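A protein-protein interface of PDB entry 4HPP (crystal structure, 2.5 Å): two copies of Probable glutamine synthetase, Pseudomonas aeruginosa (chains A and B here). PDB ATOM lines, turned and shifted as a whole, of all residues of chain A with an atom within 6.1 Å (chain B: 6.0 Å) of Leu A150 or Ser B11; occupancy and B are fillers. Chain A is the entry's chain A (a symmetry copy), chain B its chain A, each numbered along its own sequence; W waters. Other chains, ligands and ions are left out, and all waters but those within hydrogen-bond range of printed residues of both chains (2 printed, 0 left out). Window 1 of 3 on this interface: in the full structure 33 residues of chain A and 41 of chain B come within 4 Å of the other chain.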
ATOM      1  N   ALA A 146      14.796  22.890  34.574  1.00  0.00           N
ATOM      2  CA  ALA A 146      13.967  22.734  35.709  1.00  0.00           C
ATOM      3  C   ALA A 146      12.593  22.084  35.402  1.00  0.00           C
ATOM      4  O   ALA A 146      11.926  22.403  34.378  1.00  0.00           O
ATOM      5  CB  ALA A 146      13.792  24.099  36.379  1.00  0.00           C
ATOM      6  N   PHE A 148       8.790  21.388  35.166  1.00  0.00           N
ATOM      7  CA  PHE A 148       7.569  22.169  34.925  1.00  0.00           C
ATOM      8  C   PHE A 148       7.831  23.488  34.138  1.00  0.00           C
ATOM      9  O   PHE A 148       6.933  24.296  34.019  1.00  0.00           O
ATOM     10  CB  PHE A 148       6.867  22.502  36.271  1.00  0.00           C
ATOM     11  CG  PHE A 148       6.458  21.300  37.124  1.00  0.00           C
ATOM     12  CD1 PHE A 148       6.474  21.396  38.514  1.00  0.00           C
ATOM     13  CD2 PHE A 148       6.013  20.117  36.574  1.00  0.00           C
ATOM     14  CE1 PHE A 148       6.095  20.322  39.324  1.00  0.00           C
ATOM     15  CE2 PHE A 148       5.658  19.041  37.376  1.00  0.00           C
ATOM     16  CZ  PHE A 148       5.696  19.132  38.750  1.00  0.00           C
ATOM     17  N   SER A 149       9.069  23.707  33.669  1.00  0.00           N
ATOM     18  CA  SER A 149       9.549  25.021  33.297  1.00  0.00           C
ATOM     19  C   SER A 149       9.390  25.304  31.813  1.00  0.00           C
ATOM     20  O   SER A 149       9.403  24.363  30.987  1.00  0.00           O
ATOM     21  CB  SER A 149      11.009  25.276  33.794  1.00  0.00           C
ATOM     22  OG  SER A 149      11.959  24.456  33.138  1.00  0.00           O
ATOM     23  N   LEU A 150       9.220  26.596  31.482  1.00  0.00           N
ATOM     24  CA  LEU A 150       9.023  27.035  30.073  1.00  0.00           C
ATOM     25  C   LEU A 150      10.219  26.526  29.277  1.00  0.00           C
ATOM     26  O   LEU A 150      10.071  26.027  28.160  1.00  0.00           O
ATOM     27  CB  LEU A 150       8.884  28.591  29.908  1.00  0.00           C
ATOM     28  CG  LEU A 150       8.501  29.132  28.508  1.00  0.00           C
ATOM     29  CD1 LEU A 150       7.300  28.399  27.915  1.00  0.00           C
ATOM     30  CD2 LEU A 150       8.190  30.616  28.524  1.00  0.00           C
ATOM     31  N   GLN A 151      11.400  26.586  29.876  1.00  0.00           N
ATOM     32  CA  GLN A 151      12.562  26.139  29.155  1.00  0.00           C
ATOM     33  C   GLN A 151      12.482  24.692  28.806  1.00  0.00           C
ATOM     34  O   GLN A 151      12.934  24.302  27.693  1.00  0.00           O
ATOM     35  CB  GLN A 151      13.849  26.503  29.869  1.00  0.00           C
ATOM     36  CG  GLN A 151      14.267  27.952  29.656  1.00  0.00           C
ATOM     37  CD  GLN A 151      15.722  28.077  30.027  1.00  0.00           C
ATOM     38  OE1 GLN A 151      16.042  27.979  31.184  1.00  0.00           O
ATOM     39  NE2 GLN A 151      16.606  28.248  29.045  1.00  0.00           N
ATOM     40  N   ALA A 152      11.854  23.895  29.676  1.00  0.00           N
ATOM     41  CA  ALA A 152      11.792  22.437  29.394  1.00  0.00           C
ATOM     42  C   ALA A 152      10.817  22.192  28.282  1.00  0.00           C
ATOM     43  O   ALA A 152      11.038  21.303  27.464  1.00  0.00           O
ATOM     44  CB  ALA A 152      11.436  21.579  30.602  1.00  0.00           C
ATOM     45  N   GLN A 153       9.728  22.965  28.230  1.00  0.00           N
ATOM     46  CA  GLN A 153       8.822  22.833  27.101  1.00  0.00           C
ATOM     47  C   GLN A 153       9.544  23.292  25.800  1.00  0.00           C
ATOM     48  O   GLN A 153       9.496  22.594  24.783  1.00  0.00           O
ATOM     49  CB  GLN A 153       7.498  23.568  27.370  1.00  0.00           C
ATOM     50  CG  GLN A 153       6.597  23.577  26.148  1.00  0.00           C
ATOM     51  CD  GLN A 153       5.124  23.360  26.422  1.00  0.00           C
ATOM     52  OE1 GLN A 153       4.688  23.002  27.542  1.00  0.00           O
ATOM     53  NE2 GLN A 153       4.324  23.577  25.380  1.00  0.00           N
ATOM     54  N   ARG A 154      10.276  24.414  25.857  1.00  0.00           N
ATOM     55  CA  ARG A 154      11.042  24.873  24.710  1.00  0.00           C
ATOM     56  C   ARG A 154      12.087  23.920  24.223  1.00  0.00           C
ATOM     57  O   ARG A 154      12.335  23.894  23.006  1.00  0.00           O
ATOM     58  CB  ARG A 154      11.690  26.200  25.000  1.00  0.00           C
ATOM     59  CG  ARG A 154      10.647  27.286  25.152  1.00  0.00           C
ATOM     60  CD  ARG A 154       9.475  27.193  24.158  1.00  0.00           C
ATOM     61  NE  ARG A 154       9.834  27.797  22.884  1.00  0.00           N
ATOM     62  CZ  ARG A 154       8.930  28.137  21.941  1.00  0.00           C
ATOM     63  NH1 ARG A 154       7.607  27.861  22.084  1.00  0.00           N
ATOM     64  NH2 ARG A 154       9.346  28.749  20.833  1.00  0.00           N
ATOM     65  N   ALA A 155      12.710  23.148  25.136  1.00  0.00           N
ATOM     66  CA  ALA A 155      13.814  22.265  24.739  1.00  0.00           C
ATOM     67  C   ALA A 155      13.319  21.227  23.769  1.00  0.00           C
ATOM     68  O   ALA A 155      14.088  20.716  22.923  1.00  0.00           O
ATOM     69  CB  ALA A 155      14.489  21.581  25.938  1.00  0.00           C
ATOM     70  N   PRO A 179       5.626  20.098  30.317  1.00  0.00           N
ATOM     71  CA  PRO A 179       6.788  19.373  30.947  1.00  0.00           C
ATOM     72  C   PRO A 179       6.399  19.002  32.361  1.00  0.00           C
ATOM     73  O   PRO A 179       5.666  19.762  33.003  1.00  0.00           O
ATOM     74  CB  PRO A 179       7.879  20.421  31.029  1.00  0.00           C
ATOM     75  CG  PRO A 179       7.108  21.726  31.077  1.00  0.00           C
ATOM     76  CD  PRO A 179       5.828  21.562  30.282  1.00  0.00           C
ATOM     77  N   LEU B   9       1.027  26.136  20.475  1.00  0.00           N
ATOM     78  CA  LEU B   9       0.713  25.998  21.910  1.00  0.00           C
ATOM     79  C   LEU B   9       0.825  27.344  22.662  1.00  0.00           C
ATOM     80  O   LEU B   9       1.717  28.146  22.408  1.00  0.00           O
ATOM     81  CB  LEU B   9       1.566  24.906  22.548  1.00  0.00           C
ATOM     82  CG  LEU B   9       1.458  23.591  21.716  1.00  0.00           C
ATOM     83  CD1 LEU B   9       2.483  22.528  22.156  1.00  0.00           C
ATOM     84  CD2 LEU B   9       0.045  22.951  21.700  1.00  0.00           C
ATOM     85  N   VAL B  10      -0.112  27.604  23.567  1.00  0.00           N
ATOM     86  CA  VAL B  10      -0.010  28.765  24.395  1.00  0.00           C
ATOM     87  C   VAL B  10       0.323  28.299  25.803  1.00  0.00           C
ATOM     88  O   VAL B  10      -0.331  27.396  26.313  1.00  0.00           O
ATOM     89  CB  VAL B  10      -1.338  29.573  24.379  1.00  0.00           C
ATOM     90  CG1 VAL B  10      -1.226  30.705  25.372  1.00  0.00           C
ATOM     91  CG2 VAL B  10      -1.563  30.141  22.989  1.00  0.00           C
ATOM     92  N   SER B  11       1.338  28.886  26.426  1.00  0.00           N
ATOM     93  CA  SER B  11       1.589  28.588  27.819  1.00  0.00           C
ATOM     94  C   SER B  11       0.994  29.587  28.809  1.00  0.00           C
ATOM     95  O   SER B  11       0.960  30.765  28.553  1.00  0.00           O
ATOM     96  CB  SER B  11       3.090  28.458  28.070  1.00  0.00           C
ATOM     97  OG  SER B  11       3.568  27.150  27.780  1.00  0.00           O
ATOM     98  N   PHE B  12       0.493  29.090  29.940  1.00  0.00           N
ATOM     99  CA  PHE B  12       0.258  29.891  31.140  1.00  0.00           C
ATOM    100  C   PHE B  12       1.476  29.650  32.083  1.00  0.00           C
ATOM    101  O   PHE B  12       1.802  28.500  32.431  1.00  0.00           O
ATOM    102  CB  PHE B  12      -1.035  29.473  31.883  1.00  0.00           C
ATOM    103  CG  PHE B  12      -2.293  29.553  31.070  1.00  0.00           C
ATOM    104  CD1 PHE B  12      -2.396  30.399  29.939  1.00  0.00           C
ATOM    105  CD2 PHE B  12      -3.421  28.803  31.436  1.00  0.00           C
ATOM    106  CE1 PHE B  12      -3.572  30.472  29.202  1.00  0.00           C
ATOM    107  CE2 PHE B  12      -4.627  28.881  30.681  1.00  0.00           C
ATOM    108  CZ  PHE B  12      -4.680  29.701  29.561  1.00  0.00           C
ATOM    109  N   VAL B  13       2.124  30.744  32.486  1.00  0.00           N
ATOM    110  CA  VAL B  13       3.278  30.698  33.359  1.00  0.00           C
ATOM    111  C   VAL B  13       3.127  31.397  34.700  1.00  0.00           C
ATOM    112  O   VAL B  13       2.312  32.317  34.869  1.00  0.00           O
ATOM    113  CB  VAL B  13       4.516  31.250  32.656  1.00  0.00           C
ATOM    114  CG1 VAL B  13       4.755  30.488  31.377  1.00  0.00           C
ATOM    115  CG2 VAL B  13       4.378  32.732  32.355  1.00  0.00           C
ATOM    116  N   THR B  21      10.413  30.158  35.965  1.00  0.00           N
ATOM    117  CA  THR B  21       9.112  30.355  35.283  1.00  0.00           C
ATOM    118  C   THR B  21       8.659  29.031  34.747  1.00  0.00           C
ATOM    119  O   THR B  21       9.364  28.420  33.933  1.00  0.00           O
ATOM    120  CB  THR B  21       9.283  31.260  34.071  1.00  0.00           C
ATOM    121  OG1 THR B  21      10.162  32.282  34.442  1.00  0.00           O
ATOM    122  CG2 THR B  21       8.034  31.900  33.608  1.00  0.00           C
ATOM    123  N   ARG B  22       7.461  28.632  35.155  1.00  0.00           N
ATOM    124  CA  ARG B  22       6.903  27.312  34.963  1.00  0.00           C
ATOM    125  C   ARG B  22       5.491  27.466  34.415  1.00  0.00           C
ATOM    126  O   ARG B  22       4.857  28.499  34.655  1.00  0.00           O
ATOM    127  CB  ARG B  22       6.852  26.641  36.326  1.00  0.00           C
ATOM    128  CG  ARG B  22       8.259  26.249  36.806  1.00  0.00           C
ATOM    129  CD  ARG B  22       8.443  26.110  38.315  1.00  0.00           C
ATOM    130  NE  ARG B  22       9.312  24.971  38.466  1.00  0.00           N
ATOM    131  CZ  ARG B  22      10.426  24.869  39.213  1.00  0.00           C
ATOM    132  NH1 ARG B  22      10.861  25.785  40.057  1.00  0.00           N
ATOM    133  NH2 ARG B  22      11.085  23.758  39.144  1.00  0.00           N
ATOM    134  N   GLY B  23       4.987  26.467  33.682  1.00  0.00           N
ATOM    135  CA  GLY B  23       3.599  26.503  33.319  1.00  0.00           C
ATOM    136  C   GLY B  23       3.189  25.295  32.542  1.00  0.00           C
ATOM    137  O   GLY B  23       3.863  24.256  32.596  1.00  0.00           O
ATOM    138  N   ARG B  24       2.095  25.456  31.779  1.00  0.00           N
ATOM    139  CA  ARG B  24       1.442  24.369  31.084  1.00  0.00           C
ATOM    140  C   ARG B  24       0.893  24.949  29.833  1.00  0.00           C
ATOM    141  O   ARG B  24       0.568  26.129  29.816  1.00  0.00           O
ATOM    142  CB  ARG B  24       0.236  23.907  31.882  1.00  0.00           C
ATOM    143  CG  ARG B  24       0.606  23.018  33.031  1.00  0.00           C
ATOM    144  CD  ARG B  24      -0.612  22.536  33.771  1.00  0.00           C
ATOM    145  NE  ARG B  24      -0.212  22.084  35.087  1.00  0.00           N
ATOM    146  CZ  ARG B  24      -1.044  21.507  35.937  1.00  0.00           C
ATOM    147  NH1 ARG B  24      -2.304  21.352  35.565  1.00  0.00           N
ATOM    148  NH2 ARG B  24      -0.622  21.113  37.154  1.00  0.00           N
ATOM    149  N   SER B  25       0.714  24.149  28.789  1.00  0.00           N
ATOM    150  CA  SER B  25       0.270  24.770  27.553  1.00  0.00           C
ATOM    151  C   SER B  25      -0.913  24.061  26.934  1.00  0.00           C
ATOM    152  O   SER B  25      -1.227  22.899  27.281  1.00  0.00           O
ATOM    153  CB  SER B  25       1.440  24.879  26.573  1.00  0.00           C
ATOM    154  OG  SER B  25       1.676  23.621  25.969  1.00  0.00           O
ATOM    155  N   LEU B  26      -1.581  24.779  26.044  1.00  0.00           N
ATOM    156  CA  LEU B  26      -2.817  24.295  25.384  1.00  0.00           C
ATOM    157  C   LEU B  26      -2.845  24.704  23.920  1.00  0.00           C
ATOM    158  O   LEU B  26      -2.120  25.609  23.519  1.00  0.00           O
ATOM    159  CB  LEU B  26      -4.031  24.859  26.056  1.00  0.00           C
ATOM    160  CG  LEU B  26      -3.918  26.341  26.394  1.00  0.00           C
ATOM    161  CD1 LEU B  26      -5.141  27.151  25.921  1.00  0.00           C
ATOM    162  CD2 LEU B  26      -3.789  26.431  27.902  1.00  0.00           C
ATOM    163  N   LEU B  89       6.853  31.627  20.309  1.00  0.00           N
ATOM    164  CA  LEU B  89       6.809  31.654  21.728  1.00  0.00           C
ATOM    165  C   LEU B  89       5.578  32.384  22.146  1.00  0.00           C
ATOM    166  O   LEU B  89       5.479  33.579  21.948  1.00  0.00           O
ATOM    167  CB  LEU B  89       8.026  32.415  22.213  1.00  0.00           C
ATOM    168  CG  LEU B  89       8.218  32.412  23.747  1.00  0.00           C
ATOM    169  CD1 LEU B  89       8.427  31.021  24.358  1.00  0.00           C
ATOM    170  CD2 LEU B  89       9.373  33.334  24.124  1.00  0.00           C
ATOM    171  N   ASP B  90       4.637  31.695  22.741  1.00  0.00           N
ATOM    172  CA  ASP B  90       3.387  32.324  23.096  1.00  0.00           C
ATOM    173  C   ASP B  90       2.962  31.952  24.482  1.00  0.00           C
ATOM    174  O   ASP B  90       2.724  30.792  24.756  1.00  0.00           O
ATOM    175  CB  ASP B  90       2.320  31.895  22.108  1.00  0.00           C
ATOM    176  CG  ASP B  90       1.124  32.785  22.133  1.00  0.00           C
ATOM    177  OD1 ASP B  90       0.910  33.514  23.166  1.00  0.00           O
ATOM    178  OD2 ASP B  90       0.388  32.750  21.098  1.00  0.00           O
ATOM    179  N   TYR B  91       2.855  32.924  25.373  1.00  0.00           N
ATOM    180  CA  TYR B  91       2.469  32.604  26.768  1.00  0.00           C
ATOM    181  C   TYR B  91       1.990  33.866  27.462  1.00  0.00           C
ATOM    182  O   TYR B  91       2.281  34.963  27.003  1.00  0.00           O
ATOM    183  CB  TYR B  91       3.675  32.003  27.582  1.00  0.00           C
ATOM    184  CG  TYR B  91       4.765  33.019  27.765  1.00  0.00           C
ATOM    185  CD1 TYR B  91       4.735  33.940  28.810  1.00  0.00           C
ATOM    186  CD2 TYR B  91       5.826  33.080  26.876  1.00  0.00           C
ATOM    187  CE1 TYR B  91       5.772  34.890  28.968  1.00  0.00           C
ATOM    188  CE2 TYR B  91       6.864  33.997  27.030  1.00  0.00           C
ATOM    189  CZ  TYR B  91       6.824  34.922  28.063  1.00  0.00           C
ATOM    190  OH  TYR B  91       7.840  35.865  28.154  1.00  0.00           O
ATOM    191  N   LEU B  92       1.278  33.675  28.566  1.00  0.00           N
ATOM    192  CA  LEU B  92       0.715  34.715  29.414  1.00  0.00           C
ATOM    193  C   LEU B  92       1.094  34.466  30.891  1.00  0.00           C
ATOM    194  O   LEU B  92       1.083  33.311  31.369  1.00  0.00           O
ATOM    195  CB  LEU B  92      -0.820  34.669  29.353  1.00  0.00           C
ATOM    196  CG  LEU B  92      -1.558  34.899  28.050  1.00  0.00           C
ATOM    197  CD1 LEU B  92      -1.677  33.610  27.269  1.00  0.00           C
ATOM    198  CD2 LEU B  92      -2.950  35.456  28.307  1.00  0.00           C
ATOM    199  N   HIS B  93       1.391  35.550  31.610  1.00  0.00           N
ATOM    200  CA  HIS B  93       1.647  35.502  33.029  1.00  0.00           C
ATOM    201  C   HIS B  93       0.327  35.380  33.722  1.00  0.00           C
ATOM    202  O   HIS B  93      -0.688  35.939  33.262  1.00  0.00           O
ATOM    203  CB  HIS B  93       2.353  36.743  33.496  1.00  0.00           C
ATOM    204  CG  HIS B  93       3.615  37.018  32.759  1.00  0.00           C
ATOM    205  ND1 HIS B  93       4.836  36.721  33.275  1.00  0.00           N
ATOM    206  CD2 HIS B  93       3.838  37.595  31.494  1.00  0.00           C
ATOM    207  CE1 HIS B  93       5.800  37.070  32.369  1.00  0.00           C
ATOM    208  NE2 HIS B  93       5.187  37.606  31.277  1.00  0.00           N
ATOM    209  N   GLU B 207      13.284  35.061  29.504  1.00  0.00           N
ATOM    210  CA  GLU B 207      12.780  33.897  28.880  1.00  0.00           C
ATOM    211  C   GLU B 207      13.023  33.956  27.360  1.00  0.00           C
ATOM    212  O   GLU B 207      13.334  32.911  26.723  1.00  0.00           O
ATOM    213  CB  GLU B 207      11.343  33.661  29.311  1.00  0.00           C
ATOM    214  CG  GLU B 207      11.275  33.266  30.783  1.00  0.00           C
ATOM    215  CD  GLU B 207      12.048  31.989  31.031  1.00  0.00           C
ATOM    216  OE1 GLU B 207      12.822  31.943  31.978  1.00  0.00           O
ATOM    217  OE2 GLU B 207      11.859  31.028  30.269  1.00  0.00           O
HETATM  218  O   HOH W   1      11.698  28.588  31.730  1.00  0.00           O
HETATM  219  O   HOH W   2       4.311  21.697  33.838  1.00  0.00           O
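No position is printed for both chains. Of the 13 pairs that touch across the chains among the printed residues, none has its exchanged pair printed and touching as well.
Printed residues of chain A that touch a printed residue of chain B: Ala A146, Phe A148, Ser A149, Leu A150, Gln A151, Gln A153 and Arg A154. Hydrophobic or aromatic side chains of chain A that line the printed part of chain B: Ala A146 and Leu A150. Along chain A the printed residues that touch a printed residue of chain B span positions 146 to 154. Hydrophobic or aromatic side chains of chain B that line the printed part of chain A: Leu B9, Leu B89 and Tyr B91. Among the printed residues, 13 pairs touch across the chains. Among the printed residues, no Asp or Glu carboxylate lies within 4 Å of a Lys or Arg side-chain nitrogen of the other chain.
Arg B22 touches Ala A146 (NH2 to CB, 3.9 Å). Phe A148 touches Arg B22 (O to CA, 3.2 Å). Ser A149 touches Thr B21. Arg B22 touches Ser A149. CD1 of Leu A150 touches OG of Ser B11 (3.9 Å). Leu A150 touches Tyr B91 (CD2 to CD2, 3.8 Å). CB of Leu A150 touches OE2 of Glu B207 (3.9 Å). Glu B207 touches Gln A151. Gln A153 touches Leu B9. Leu B89 touches Arg A154 (CD1 to CZ, 3.8 Å).
Of the printed residues of chain B, Ser A149 touches Thr B21 and Arg B22. Leu A150 touches four residues of chain B. Of the printed residues of chain B, Gln A151 touches Glu B207 (3.95 Å). Ala A155 touches none of the printed residues of chain B. Of chain A, only Leu A150 (3.9 Å) comes within 4 Å of Ser B11. Of the printed residues of chain A, Arg B22 touches Ala A146, Phe A148 and Ser A149. Printed residues of chain A within 4 Å of Tyr B91: Leu A150 (3.8 Å). Printed residues of chain A within 4 Å of Glu B207: Leu A150 and Gln A151. The nearest residue of chain B that does not touch Leu A150 is Leu B89 (4.2 Å). The nearest residue of chain A that does not touch Ser B11 is Gln A153 (4.3 Å).
Water W2 bridges O of Pro A179 (2.5 Å) and O of Gly B23 (2.9 Å). Water W1 lies within hydrogen-bond range of the backbone NH (N) of Gln A151 (2.7 Å), the side-chain carboxylate (OE2) of Glu B207 (2.8 Å), the backbone NH (N) of Leu A150 (3.2 Å) and the backbone carbonyl oxygen (O) of Thr B21 (3.2 Å).
O of Asp B90 sits at hydrogen-bond distance from N of Ser B11 (2.9 Å). The backbone carbonyl oxygen (O) of Ser B11 sits at hydrogen-bond distance from the backbone NH (N) of Leu B92.
O of Thr B21 lies within hydrogen-bond range of N of Leu A150, at 3.1 Å. The backbone carbonyl oxygen of Phe A148 sits at hydrogen-bond distance from the backbone NH of Gly B23, 2.9 Å away. The side-chain hydroxyl (OG) of Ser B25 sits at hydrogen-bond distance from the side-chain amide nitrogen (NE2) of Gln A153.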
